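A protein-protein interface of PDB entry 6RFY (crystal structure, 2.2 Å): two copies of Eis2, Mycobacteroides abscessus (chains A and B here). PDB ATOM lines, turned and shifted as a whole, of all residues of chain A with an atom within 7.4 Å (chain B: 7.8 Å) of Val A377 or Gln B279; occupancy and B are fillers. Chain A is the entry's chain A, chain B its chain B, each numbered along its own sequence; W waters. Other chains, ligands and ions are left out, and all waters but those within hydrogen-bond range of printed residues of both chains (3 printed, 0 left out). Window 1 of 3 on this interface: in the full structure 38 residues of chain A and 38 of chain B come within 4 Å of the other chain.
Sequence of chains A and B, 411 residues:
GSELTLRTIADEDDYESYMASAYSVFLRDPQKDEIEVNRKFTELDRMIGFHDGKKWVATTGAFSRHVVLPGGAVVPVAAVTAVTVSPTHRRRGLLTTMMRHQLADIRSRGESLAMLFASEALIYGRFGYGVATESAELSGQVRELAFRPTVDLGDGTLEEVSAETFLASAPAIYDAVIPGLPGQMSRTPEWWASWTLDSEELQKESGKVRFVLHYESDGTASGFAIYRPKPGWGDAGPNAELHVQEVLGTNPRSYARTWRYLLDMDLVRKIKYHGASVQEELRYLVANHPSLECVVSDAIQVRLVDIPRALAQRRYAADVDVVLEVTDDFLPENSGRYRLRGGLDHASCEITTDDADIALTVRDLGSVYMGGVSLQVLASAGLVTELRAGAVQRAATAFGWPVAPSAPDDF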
ATOM      1  N   GLU A 134       0.296  28.085  -4.237  1.00  0.00           N
ATOM      2  CA  GLU A 134      -1.041  27.865  -3.714  1.00  0.00           C
ATOM      3  C   GLU A 134      -1.516  29.110  -2.978  1.00  0.00           C
ATOM      4  O   GLU A 134      -0.728  29.988  -2.615  1.00  0.00           O
ATOM      5  CB  GLU A 134      -1.081  26.657  -2.772  1.00  0.00           C
ATOM      6  CG  GLU A 134      -0.586  25.370  -3.398  1.00  0.00           C
ATOM      7  CD  GLU A 134      -0.652  24.200  -2.443  1.00  0.00           C
ATOM      8  OE1 GLU A 134      -1.457  23.279  -2.689  1.00  0.00           O
ATOM      9  OE2 GLU A 134       0.097  24.202  -1.443  1.00  0.00           O
ATOM     10  N   GLY A 372       7.103  26.304  -3.571  1.00  0.00           N
ATOM     11  CA  GLY A 372       5.803  26.010  -2.998  1.00  0.00           C
ATOM     12  C   GLY A 372       5.369  24.564  -3.123  1.00  0.00           C
ATOM     13  O   GLY A 372       4.341  24.170  -2.566  1.00  0.00           O
ATOM     14  N   VAL A 373       6.147  23.762  -3.847  1.00  0.00           N
ATOM     15  CA  VAL A 373       5.871  22.340  -4.037  1.00  0.00           C
ATOM     16  C   VAL A 373       7.188  21.596  -3.878  1.00  0.00           C
ATOM     17  O   VAL A 373       8.167  21.909  -4.564  1.00  0.00           O
ATOM     18  CB  VAL A 373       5.243  22.033  -5.410  1.00  0.00           C
ATOM     19  CG1 VAL A 373       4.960  20.543  -5.540  1.00  0.00           C
ATOM     20  CG2 VAL A 373       3.961  22.838  -5.618  1.00  0.00           C
ATOM     21  N   SER A 374       7.217  20.617  -2.977  1.00  0.00           N
ATOM     22  CA  SER A 374       8.446  19.888  -2.699  1.00  0.00           C
ATOM     23  C   SER A 374       8.775  18.919  -3.827  1.00  0.00           C
ATOM     24  O   SER A 374       7.934  18.114  -4.238  1.00  0.00           O
ATOM     25  CB  SER A 374       8.325  19.130  -1.381  1.00  0.00           C
ATOM     26  OG  SER A 374       9.413  18.238  -1.223  1.00  0.00           O
ATOM     27  N   LEU A 375      10.012  18.994  -4.325  1.00  0.00           N
ATOM     28  CA  LEU A 375      10.471  18.023  -5.311  1.00  0.00           C
ATOM     29  C   LEU A 375      10.445  16.605  -4.749  1.00  0.00           C
ATOM     30  O   LEU A 375      10.184  15.649  -5.488  1.00  0.00           O
ATOM     31  CB  LEU A 375      11.877  18.393  -5.784  1.00  0.00           C
ATOM     32  CG  LEU A 375      12.509  17.602  -6.930  1.00  0.00           C
ATOM     33  CD1 LEU A 375      11.755  17.827  -8.239  1.00  0.00           C
ATOM     34  CD2 LEU A 375      13.969  17.988  -7.084  1.00  0.00           C
ATOM     35  N   GLN A 376      10.676  16.454  -3.441  1.00  0.00           N
ATOM     36  CA  GLN A 376      10.644  15.130  -2.823  1.00  0.00           C
ATOM     37  C   GLN A 376       9.268  14.489  -2.946  1.00  0.00           C
ATOM     38  O   GLN A 376       9.156  13.285  -3.205  1.00  0.00           O
ATOM     39  CB  GLN A 376      11.049  15.234  -1.353  1.00  0.00           C
ATOM     40  CG  GLN A 376      10.982  13.924  -0.588  1.00  0.00           C
ATOM     41  CD  GLN A 376      11.958  12.887  -1.105  1.00  0.00           C
ATOM     42  OE1 GLN A 376      13.150  12.936  -0.802  1.00  0.00           O
ATOM     43  NE2 GLN A 376      11.453  11.936  -1.885  1.00  0.00           N
ATOM     44  N   VAL A 377       8.207  15.276  -2.762  1.00  0.00           N
ATOM     45  CA  VAL A 377       6.858  14.729  -2.863  1.00  0.00           C
ATOM     46  C   VAL A 377       6.548  14.321  -4.299  1.00  0.00           C
ATOM     47  O   VAL A 377       5.932  13.276  -4.540  1.00  0.00           O
ATOM     48  CB  VAL A 377       5.829  15.733  -2.315  1.00  0.00           C
ATOM     49  CG1 VAL A 377       4.450  15.121  -2.345  1.00  0.00           C
ATOM     50  CG2 VAL A 377       6.194  16.143  -0.896  1.00  0.00           C
ATOM     51  N   LEU A 378       6.956  15.138  -5.276  1.00  0.00           N
ATOM     52  CA  LEU A 378       6.765  14.764  -6.676  1.00  0.00           C
ATOM     53  C   LEU A 378       7.475  13.453  -6.999  1.00  0.00           C
ATOM     54  O   LEU A 378       6.971  12.642  -7.786  1.00  0.00           O
ATOM     55  CB  LEU A 378       7.265  15.880  -7.594  1.00  0.00           C
ATOM     56  CG  LEU A 378       6.562  17.239  -7.547  1.00  0.00           C
ATOM     57  CD1 LEU A 378       7.050  18.115  -8.688  1.00  0.00           C
ATOM     58  CD2 LEU A 378       5.044  17.081  -7.604  1.00  0.00           C
ATOM     59  N   ALA A 379       8.640  13.221  -6.390  1.00  0.00           N
ATOM     60  CA  ALA A 379       9.352  11.968  -6.615  1.00  0.00           C
ATOM     61  C   ALA A 379       8.642  10.803  -5.936  1.00  0.00           C
ATOM     62  O   ALA A 379       8.486   9.732  -6.534  1.00  0.00           O
ATOM     63  CB  ALA A 379      10.794  12.084  -6.122  1.00  0.00           C
ATOM     64  N   SER A 380       8.204  10.995  -4.689  1.00  0.00           N
ATOM     65  CA  SER A 380       7.464   9.943  -4.000  1.00  0.00           C
ATOM     66  C   SER A 380       6.173   9.601  -4.732  1.00  0.00           C
ATOM     67  O   SER A 380       5.680   8.472  -4.627  1.00  0.00           O
ATOM     68  CB  SER A 380       7.164  10.363  -2.560  1.00  0.00           C
ATOM     69  OG  SER A 380       8.351  10.438  -1.792  1.00  0.00           O
ATOM     70  N   ALA A 381       5.607  10.561  -5.466  1.00  0.00           N
ATOM     71  CA  ALA A 381       4.396  10.314  -6.237  1.00  0.00           C
ATOM     72  C   ALA A 381       4.664   9.551  -7.528  1.00  0.00           C
ATOM     73  O   ALA A 381       3.718   9.028  -8.128  1.00  0.00           O
ATOM     74  CB  ALA A 381       3.698  11.635  -6.557  1.00  0.00           C
ATOM     75  N   GLY A 382       5.919   9.472  -7.969  1.00  0.00           N
ATOM     76  CA  GLY A 382       6.247   8.837  -9.226  1.00  0.00           C
ATOM     77  C   GLY A 382       6.349   9.775 -10.409  1.00  0.00           C
ATOM     78  O   GLY A 382       6.562   9.307 -11.533  1.00  0.00           O
ATOM     79  N   LEU A 383       6.193  11.082 -10.195  1.00  0.00           N
ATOM     80  CA  LEU A 383       6.249  12.038 -11.293  1.00  0.00           C
ATOM     81  C   LEU A 383       7.677  12.443 -11.625  1.00  0.00           C
ATOM     82  O   LEU A 383       7.961  12.814 -12.769  1.00  0.00           O
ATOM     83  CB  LEU A 383       5.420  13.274 -10.945  1.00  0.00           C
ATOM     84  CG  LEU A 383       3.950  13.000 -10.624  1.00  0.00           C
ATOM     85  CD1 LEU A 383       3.319  14.207  -9.959  1.00  0.00           C
ATOM     86  CD2 LEU A 383       3.190  12.629 -11.886  1.00  0.00           C
ATOM     87  N   VAL A 384       8.569  12.399 -10.640  1.00  0.00           N
ATOM     88  CA  VAL A 384       9.982  12.712 -10.804  1.00  0.00           C
ATOM     89  C   VAL A 384      10.792  11.476 -10.431  1.00  0.00           C
ATOM     90  O   VAL A 384      10.412  10.717  -9.533  1.00  0.00           O
ATOM     91  CB  VAL A 384      10.380  13.934  -9.945  1.00  0.00           C
ATOM     92  CG1 VAL A 384      11.881  14.145  -9.942  1.00  0.00           C
ATOM     93  CG2 VAL A 384       9.665  15.181 -10.449  1.00  0.00           C
ATOM     94  N   VAL A 392      17.577  13.785  -4.704  1.00  0.00           N
ATOM     95  CA  VAL A 392      16.256  14.412  -4.640  1.00  0.00           C
ATOM     96  C   VAL A 392      16.056  15.117  -3.304  1.00  0.00           C
ATOM     97  O   VAL A 392      15.535  16.238  -3.251  1.00  0.00           O
ATOM     98  CB  VAL A 392      15.153  13.372  -4.908  1.00  0.00           C
ATOM     99  CG1 VAL A 392      13.796  13.912  -4.489  1.00  0.00           C
ATOM    100  CG2 VAL A 392      15.129  13.009  -6.381  1.00  0.00           C
ATOM    101  N   ALA A 396      15.430  18.985  -3.111  1.00  0.00           N
ATOM    102  CA  ALA A 396      14.123  19.439  -2.649  1.00  0.00           C
ATOM    103  C   ALA A 396      14.278  20.526  -1.593  1.00  0.00           C
ATOM    104  O   ALA A 396      13.590  21.551  -1.635  1.00  0.00           O
ATOM    105  CB  ALA A 396      13.317  18.261  -2.102  1.00  0.00           C
ATOM    106  N   GLU B 134       0.177  19.188  11.013  1.00  0.00           N
ATOM    107  CA  GLU B 134      -1.158  19.432  10.502  1.00  0.00           C
ATOM    108  C   GLU B 134      -1.647  18.210   9.738  1.00  0.00           C
ATOM    109  O   GLU B 134      -0.867  17.333   9.356  1.00  0.00           O
ATOM    110  CB  GLU B 134      -1.198  20.661   9.584  1.00  0.00           C
ATOM    111  CG  GLU B 134      -0.693  21.934  10.221  1.00  0.00           C
ATOM    112  CD  GLU B 134      -0.768  23.114   9.273  1.00  0.00           C
ATOM    113  OE1 GLU B 134      -1.590  24.020   9.521  1.00  0.00           O
ATOM    114  OE2 GLU B 134      -0.023  23.124   8.270  1.00  0.00           O
ATOM    115  N   SER B 135      -2.958  18.161   9.523  1.00  0.00           N
ATOM    116  CA  SER B 135      -3.577  17.140   8.697  1.00  0.00           C
ATOM    117  C   SER B 135      -4.496  17.814   7.690  1.00  0.00           C
ATOM    118  O   SER B 135      -4.927  18.954   7.874  1.00  0.00           O
ATOM    119  CB  SER B 135      -4.361  16.116   9.533  1.00  0.00           C
ATOM    120  OG  SER B 135      -5.407  16.735  10.258  1.00  0.00           O
ATOM    121  N   ALA B 136      -4.771  17.101   6.604  1.00  0.00           N
ATOM    122  CA  ALA B 136      -5.612  17.602   5.530  1.00  0.00           C
ATOM    123  C   ALA B 136      -6.819  16.693   5.367  1.00  0.00           C
ATOM    124  O   ALA B 136      -6.686  15.465   5.372  1.00  0.00           O
ATOM    125  CB  ALA B 136      -4.836  17.690   4.214  1.00  0.00           C
ATOM    126  N   LEU B 138      -9.197  15.560   2.617  1.00  0.00           N
ATOM    127  CA  LEU B 138      -9.296  15.512   1.167  1.00  0.00           C
ATOM    128  C   LEU B 138     -10.619  14.877   0.767  1.00  0.00           C
ATOM    129  O   LEU B 138     -11.019  13.853   1.329  1.00  0.00           O
ATOM    130  CB  LEU B 138      -8.129  14.724   0.567  1.00  0.00           C
ATOM    131  CG  LEU B 138      -6.723  15.165   0.989  1.00  0.00           C
ATOM    132  CD1 LEU B 138      -5.670  14.225   0.421  1.00  0.00           C
ATOM    133  CD2 LEU B 138      -6.448  16.601   0.554  1.00  0.00           C
ATOM    134  N   LEU B 181       8.345   8.952   7.064  1.00  0.00           N
ATOM    135  CA  LEU B 181       7.127   9.703   7.366  1.00  0.00           C
ATOM    136  C   LEU B 181       7.181  10.159   8.819  1.00  0.00           C
ATOM    137  O   LEU B 181       6.589   9.517   9.699  1.00  0.00           O
ATOM    138  CB  LEU B 181       5.877   8.864   7.118  1.00  0.00           C
ATOM    139  CG  LEU B 181       5.633   8.352   5.700  1.00  0.00           C
ATOM    140  CD1 LEU B 181       4.488   7.351   5.698  1.00  0.00           C
ATOM    141  CD2 LEU B 181       5.343   9.510   4.759  1.00  0.00           C
ATOM    142  N   TYR B 255       0.837   2.486  -4.238  1.00  0.00           N
ATOM    143  CA  TYR B 255       0.049   3.576  -3.673  1.00  0.00           C
ATOM    144  C   TYR B 255      -0.967   4.095  -4.685  1.00  0.00           C
ATOM    145  O   TYR B 255      -2.158   4.224  -4.378  1.00  0.00           O
ATOM    146  CB  TYR B 255       0.976   4.699  -3.205  1.00  0.00           C
ATOM    147  CG  TYR B 255       0.262   5.895  -2.612  1.00  0.00           C
ATOM    148  CD1 TYR B 255      -0.146   6.956  -3.414  1.00  0.00           C
ATOM    149  CD2 TYR B 255       0.009   5.971  -1.246  1.00  0.00           C
ATOM    150  CE1 TYR B 255      -0.797   8.049  -2.872  1.00  0.00           C
ATOM    151  CE2 TYR B 255      -0.639   7.061  -0.698  1.00  0.00           C
ATOM    152  CZ  TYR B 255      -1.037   8.098  -1.516  1.00  0.00           C
ATOM    153  OH  TYR B 255      -1.680   9.185  -0.976  1.00  0.00           O
ATOM    154  N   ALA B 276      -5.388  13.008   6.490  1.00  0.00           N
ATOM    155  CA  ALA B 276      -4.281  12.763   5.585  1.00  0.00           C
ATOM    156  C   ALA B 276      -3.152  13.756   5.851  1.00  0.00           C
ATOM    157  O   ALA B 276      -3.290  14.709   6.622  1.00  0.00           O
ATOM    158  CB  ALA B 276      -4.742  12.861   4.133  1.00  0.00           C
ATOM    159  N   SER B 277      -2.015  13.516   5.209  1.00  0.00           N
ATOM    160  CA  SER B 277      -0.938  14.491   5.249  1.00  0.00           C
ATOM    161  C   SER B 277      -1.294  15.694   4.384  1.00  0.00           C
ATOM    162  O   SER B 277      -1.937  15.565   3.340  1.00  0.00           O
ATOM    163  CB  SER B 277       0.370  13.874   4.762  1.00  0.00           C
ATOM    164  OG  SER B 277       1.260  14.884   4.324  1.00  0.00           O
ATOM    165  N   VAL B 278      -0.865  16.880   4.826  1.00  0.00           N
ATOM    166  CA  VAL B 278      -1.051  18.076   4.014  1.00  0.00           C
ATOM    167  C   VAL B 278      -0.273  17.979   2.708  1.00  0.00           C
ATOM    168  O   VAL B 278      -0.539  18.738   1.768  1.00  0.00           O
ATOM    169  CB  VAL B 278      -0.646  19.336   4.807  1.00  0.00           C
ATOM    170  CG1 VAL B 278      -1.450  19.422   6.097  1.00  0.00           C
ATOM    171  CG2 VAL B 278       0.842  19.322   5.103  1.00  0.00           C
ATOM    172  N   GLN B 279       0.680  17.056   2.624  1.00  0.00           N
ATOM    173  CA  GLN B 279       1.391  16.744   1.394  1.00  0.00           C
ATOM    174  C   GLN B 279       1.119  15.303   0.979  1.00  0.00           C
ATOM    175  O   GLN B 279       2.003  14.602   0.479  1.00  0.00           O
ATOM    176  CB  GLN B 279       2.888  17.006   1.543  1.00  0.00           C
ATOM    177  CG  GLN B 279       3.241  18.484   1.637  1.00  0.00           C
ATOM    178  CD  GLN B 279       4.732  18.721   1.779  1.00  0.00           C
ATOM    179  OE1 GLN B 279       5.506  17.783   1.977  1.00  0.00           O
ATOM    180  NE2 GLN B 279       5.143  19.980   1.682  1.00  0.00           N
ATOM    181  N   GLU B 280      -0.115  14.847   1.202  1.00  0.00           N
ATOM    182  CA  GLU B 280      -0.543  13.525   0.762  1.00  0.00           C
ATOM    183  C   GLU B 280      -0.278  13.339  -0.723  1.00  0.00           C
ATOM    184  O   GLU B 280      -0.639  14.188  -1.544  1.00  0.00           O
ATOM    185  CB  GLU B 280      -2.031  13.323   1.059  1.00  0.00           C
ATOM    186  CG  GLU B 280      -2.516  11.887   0.859  1.00  0.00           C
ATOM    187  CD  GLU B 280      -2.002  10.923   1.913  1.00  0.00           C
ATOM    188  OE1 GLU B 280      -1.886  11.321   3.092  1.00  0.00           O
ATOM    189  OE2 GLU B 280      -1.704   9.763   1.554  1.00  0.00           O
ATOM    190  N   GLU B 281       0.363  12.216  -1.059  1.00  0.00           N
ATOM    191  CA  GLU B 281       0.786  11.973  -2.434  1.00  0.00           C
ATOM    192  C   GLU B 281      -0.391  12.027  -3.400  1.00  0.00           C
ATOM    193  O   GLU B 281      -0.221  12.409  -4.564  1.00  0.00           O
ATOM    194  CB  GLU B 281       1.476  10.610  -2.521  1.00  0.00           C
ATOM    195  CG  GLU B 281       2.723  10.465  -1.656  1.00  0.00           C
ATOM    196  CD  GLU B 281       3.825  11.434  -2.015  1.00  0.00           C
ATOM    197  OE1 GLU B 281       3.906  11.833  -3.195  1.00  0.00           O
ATOM    198  OE2 GLU B 281       4.616  11.795  -1.117  1.00  0.00           O
ATOM    199  N   LEU B 282      -1.586  11.647  -2.931  1.00  0.00           N
ATOM    200  CA  LEU B 282      -2.794  11.722  -3.752  1.00  0.00           C
ATOM    201  C   LEU B 282      -3.012  13.117  -4.328  1.00  0.00           C
ATOM    202  O   LEU B 282      -3.446  13.260  -5.478  1.00  0.00           O
ATOM    203  CB  LEU B 282      -4.009  11.292  -2.926  1.00  0.00           C
ATOM    204  CG  LEU B 282      -5.369  11.409  -3.621  1.00  0.00           C
ATOM    205  CD1 LEU B 282      -5.455  10.429  -4.785  1.00  0.00           C
ATOM    206  CD2 LEU B 282      -6.517  11.186  -2.639  1.00  0.00           C
ATOM    207  N   ARG B 283      -2.709  14.161  -3.549  1.00  0.00           N
ATOM    208  CA  ARG B 283      -2.946  15.527  -4.014  1.00  0.00           C
ATOM    209  C   ARG B 283      -2.212  15.829  -5.314  1.00  0.00           C
ATOM    210  O   ARG B 283      -2.701  16.618  -6.132  1.00  0.00           O
ATOM    211  CB  ARG B 283      -2.530  16.536  -2.943  1.00  0.00           C
ATOM    212  CG  ARG B 283      -3.302  16.456  -1.637  1.00  0.00           C
ATOM    213  CD  ARG B 283      -2.910  17.629  -0.751  1.00  0.00           C
ATOM    214  NE  ARG B 283      -3.258  18.896  -1.391  1.00  0.00           N
ATOM    215  CZ  ARG B 283      -2.659  20.058  -1.145  1.00  0.00           C
ATOM    216  NH1 ARG B 283      -1.665  20.132  -0.269  1.00  0.00           N
ATOM    217  NH2 ARG B 283      -3.054  21.148  -1.788  1.00  0.00           N
ATOM    218  N   TYR B 284      -1.049  15.216  -5.528  1.00  0.00           N
ATOM    219  CA  TYR B 284      -0.249  15.498  -6.713  1.00  0.00           C
ATOM    220  C   TYR B 284      -0.437  14.463  -7.813  1.00  0.00           C
ATOM    221  O   TYR B 284      -0.062  14.729  -8.960  1.00  0.00           O
ATOM    222  CB  TYR B 284       1.231  15.604  -6.321  1.00  0.00           C
ATOM    223  CG  TYR B 284       1.426  16.545  -5.154  1.00  0.00           C
ATOM    224  CD1 TYR B 284       1.541  17.915  -5.353  1.00  0.00           C
ATOM    225  CD2 TYR B 284       1.449  16.069  -3.850  1.00  0.00           C
ATOM    226  CE1 TYR B 284       1.698  18.782  -4.285  1.00  0.00           C
ATOM    227  CE2 TYR B 284       1.601  16.926  -2.778  1.00  0.00           C
ATOM    228  CZ  TYR B 284       1.728  18.282  -3.002  1.00  0.00           C
ATOM    229  OH  TYR B 284       1.883  19.138  -1.937  1.00  0.00           O
ATOM    230  N   LEU B 285      -1.041  13.314  -7.503  1.00  0.00           N
ATOM    231  CA  LEU B 285      -1.412  12.366  -8.547  1.00  0.00           C
ATOM    232  C   LEU B 285      -2.612  12.867  -9.341  1.00  0.00           C
ATOM    233  O   LEU B 285      -2.686  12.668 -10.561  1.00  0.00           O
ATOM    234  CB  LEU B 285      -1.719  11.003  -7.930  1.00  0.00           C
ATOM    235  CG  LEU B 285      -0.585  10.301  -7.186  1.00  0.00           C
ATOM    236  CD1 LEU B 285      -1.115   9.058  -6.494  1.00  0.00           C
ATOM    237  CD2 LEU B 285       0.539   9.945  -8.145  1.00  0.00           C
ATOM    238  N   CYS B 294      -9.012  20.466  -0.255  1.00  0.00           N
ATOM    239  CA  CYS B 294      -7.992  20.266   0.768  1.00  0.00           C
ATOM    240  C   CYS B 294      -8.203  21.278   1.888  1.00  0.00           C
ATOM    241  O   CYS B 294      -7.999  22.480   1.688  1.00  0.00           O
ATOM    242  CB  CYS B 294      -6.589  20.395   0.172  1.00  0.00           C
ATOM    243  SG  CYS B 294      -5.263  20.182   1.369  1.00  0.00           S
ATOM    244  N   VAL B 296      -6.946  22.224   5.670  1.00  0.00           N
ATOM    245  CA  VAL B 296      -5.813  21.998   6.562  1.00  0.00           C
ATOM    246  C   VAL B 296      -6.195  22.410   7.976  1.00  0.00           C
ATOM    247  O   VAL B 296      -6.782  23.479   8.186  1.00  0.00           O
ATOM    248  CB  VAL B 296      -4.568  22.774   6.081  1.00  0.00           C
ATOM    249  CG1 VAL B 296      -3.415  22.603   7.060  1.00  0.00           C
ATOM    250  CG2 VAL B 296      -4.156  22.305   4.695  1.00  0.00           C
ATOM    251  N   GLY B 371       9.305  19.812  11.640  1.00  0.00           N
ATOM    252  CA  GLY B 371       9.408  20.302  10.281  1.00  0.00           C
ATOM    253  C   GLY B 371       8.097  20.665   9.624  1.00  0.00           C
ATOM    254  O   GLY B 371       8.060  20.812   8.397  1.00  0.00           O
ATOM    255  N   TRP B 401      11.813  20.024   6.629  1.00  0.00           N
ATOM    256  CA  TRP B 401      12.085  18.671   6.163  1.00  0.00           C
ATOM    257  C   TRP B 401      11.419  18.482   4.811  1.00  0.00           C
ATOM    258  O   TRP B 401      10.315  19.004   4.607  1.00  0.00           O
ATOM    259  CB  TRP B 401      11.580  17.629   7.171  1.00  0.00           C
ATOM    260  CG  TRP B 401      12.174  16.270   6.981  1.00  0.00           C
ATOM    261  CD1 TRP B 401      11.519  15.129   6.617  1.00  0.00           C
ATOM    262  CD2 TRP B 401      13.558  15.914   7.112  1.00  0.00           C
ATOM    263  NE1 TRP B 401      12.407  14.080   6.533  1.00  0.00           N
ATOM    264  CE2 TRP B 401      13.665  14.538   6.829  1.00  0.00           C
ATOM    265  CE3 TRP B 401      14.715  16.626   7.447  1.00  0.00           C
ATOM    266  CZ2 TRP B 401      14.883  13.858   6.872  1.00  0.00           C
ATOM    267  CZ3 TRP B 401      15.923  15.948   7.491  1.00  0.00           C
ATOM    268  CH2 TRP B 401      15.998  14.578   7.204  1.00  0.00           C
ATOM    269  N   PRO B 402      12.043  17.759   3.875  1.00  0.00           N
ATOM    270  CA  PRO B 402      11.434  17.601   2.542  1.00  0.00           C
ATOM    271  C   PRO B 402      10.115  16.855   2.556  1.00  0.00           C
ATOM    272  O   PRO B 402       9.318  17.021   1.623  1.00  0.00           O
ATOM    273  CB  PRO B 402      12.501  16.826   1.755  1.00  0.00           C
ATOM    274  CG  PRO B 402      13.772  17.053   2.499  1.00  0.00           C
ATOM    275  CD  PRO B 402      13.390  17.171   3.939  1.00  0.00           C
ATOM    276  N   VAL B 403       9.863  16.035   3.572  1.00  0.00           N
ATOM    277  CA  VAL B 403       8.597  15.329   3.737  1.00  0.00           C
ATOM    278  C   VAL B 403       7.906  15.918   4.956  1.00  0.00           C
ATOM    279  O   VAL B 403       8.454  15.890   6.065  1.00  0.00           O
ATOM    280  CB  VAL B 403       8.798  13.815   3.897  1.00  0.00           C
ATOM    281  CG1 VAL B 403       7.467  13.136   4.189  1.00  0.00           C
ATOM    282  CG2 VAL B 403       9.443  13.229   2.651  1.00  0.00           C
ATOM    283  N   ALA B 404       6.706  16.452   4.754  1.00  0.00           N
ATOM    284  CA  ALA B 404       5.976  17.047   5.855  1.00  0.00           C
ATOM    285  C   ALA B 404       5.605  15.978   6.880  1.00  0.00           C
ATOM    286  O   ALA B 404       5.331  14.828   6.521  1.00  0.00           O
ATOM    287  CB  ALA B 404       4.716  17.741   5.344  1.00  0.00           C
ATOM    288  N   PRO B 405       5.604  16.322   8.163  1.00  0.00           N
ATOM    289  CA  PRO B 405       5.117  15.382   9.174  1.00  0.00           C
ATOM    290  C   PRO B 405       3.625  15.146   9.011  1.00  0.00           C
ATOM    291  O   PRO B 405       2.898  15.957   8.433  1.00  0.00           O
ATOM    292  CB  PRO B 405       5.429  16.084  10.497  1.00  0.00           C
ATOM    293  CG  PRO B 405       5.396  17.538  10.147  1.00  0.00           C
ATOM    294  CD  PRO B 405       5.949  17.631   8.745  1.00  0.00           C
ATOM    295  N   SER B 406       3.171  14.001   9.516  1.00  0.00           N
ATOM    296  CA  SER B 406       1.779  13.607   9.366  1.00  0.00           C
ATOM    297  C   SER B 406       1.273  13.010  10.670  1.00  0.00           C
ATOM    298  O   SER B 406       2.049  12.580  11.528  1.00  0.00           O
ATOM    299  CB  SER B 406       1.592  12.609   8.213  1.00  0.00           C
ATOM    300  OG  SER B 406       2.515  11.542   8.304  1.00  0.00           O
HETATM  301  O   HOH W   1      -0.672  22.853   0.413  1.00  0.00           O
HETATM  302  O   HOH W   2       1.505  22.006  -2.945  1.00  0.00           O
HETATM  303  O   HOH W   3       4.533  20.244  -1.376  1.00  0.00           O
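The guanidinium group of Arg B283 is in salt-bridge range of the side-chain carboxylate of Glu A134 (2.8 Å).
O of Pro B402 lies within hydrogen-bond range of OG of Ser A374 (3.1 Å).
N of Ala A381 is in hydrogen-bond range of OE1 of Glu B281, 3.1 Å away.
The side-chain carboxylate of Glu B281 sits close to the backbone carbonyl oxygen of Val A377, at 2.8 Å.
OG of Ser A374 is in hydrogen-bond range of N of Gln A376 (3.1 Å).
OG of Ser A380 is in hydrogen-bond range of O of Gln A376, at 3.3 Å.
The backbone carbonyl oxygen (O) of Leu A378 sits at hydrogen-bond distance from the backbone NH (N) of Leu A383 (3.0 Å).
The backbone NH (N) of Ala B404 is in hydrogen-bond range of the side-chain amide oxygen (OE1) of Gln B279, at 3.3 Å.
NE of Arg B283 sits close to SG of Cys B294 (3.6 Å).
Val A373 touches Tyr B284.
Pro B402 touches Gln A376 (CB to CB, 3.8 Å).
CG of Gln A376 touches CG2 of Val B403, 3.7 Å away.
Gln B279 touches Val A377 (OE1 to CG2, 3.4 Å).
CG1 of Val A377 touches CE2 of Tyr B284, 3.4 Å away.
OE2 of Glu B281 touches CB of Ser A380, at 3.3 Å.
Ala A381 touches Leu B285 (O to CD2, 3.3 Å).
Leu A383 touches Tyr B284 (CD1 to O, 3.6 Å).
Printed residues of chain B within 4 Å of Ser A374: Pro B402.
Of the printed residues of chain B, Gln A376 touches Pro B402 (3.8 Å) and Val B403 (3.7 Å).
Of chain B, only Gln B279, Glu B281 and Tyr B284 come within 4 Å of Val A377.
Val A392 touches none of the printed residues of chain B.
Gln B279 touches just one residue of chain A: Val A377 (3.4 Å).
Of the printed residues of chain A, Tyr B284 touches Val A373, Val A377 and Leu A383.
Trp B401 touches none of the printed residues of chain A.
Of the printed residues of chain A, Pro B402 touches Ser A374 (3.1 Å) and Gln A376 (3.8 Å).
The nearest residue of chain A that does not touch Gln B279 is Ser A374 (4.5 Å).
Of the 16 printed residues of chain A, 8 touch a printed residue of chain B.
Hydrophobic or aromatic side chains of chain A within 4 Å of the printed part of chain B: Val A373, Val A377, Ala A381 and Leu A383.
Of the 25 printed residues of chain B, 7 touch a printed residue of chain A.
Hydrophobic or aromatic side chains of chain B that line the printed part of chain A: Tyr B284, Leu B285, Pro B402 and Val B403.
Among the printed residues, 12 pairs touch across the chains.
1 position is printed for both chains.
Water W1 lies within hydrogen-bond range of OE2 of Glu A134 (2.4 Å) and NH1 of Arg B283 (3.0 Å).
Water W3 lies within hydrogen-bond range of OH of Tyr B284 (2.9 Å), NE2 of Gln B279 (3.1 Å) and N of Ser A374 (3.1 Å).
Water W2 lies within hydrogen-bond range of OE2 of Glu A134 and OH of Tyr B284.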
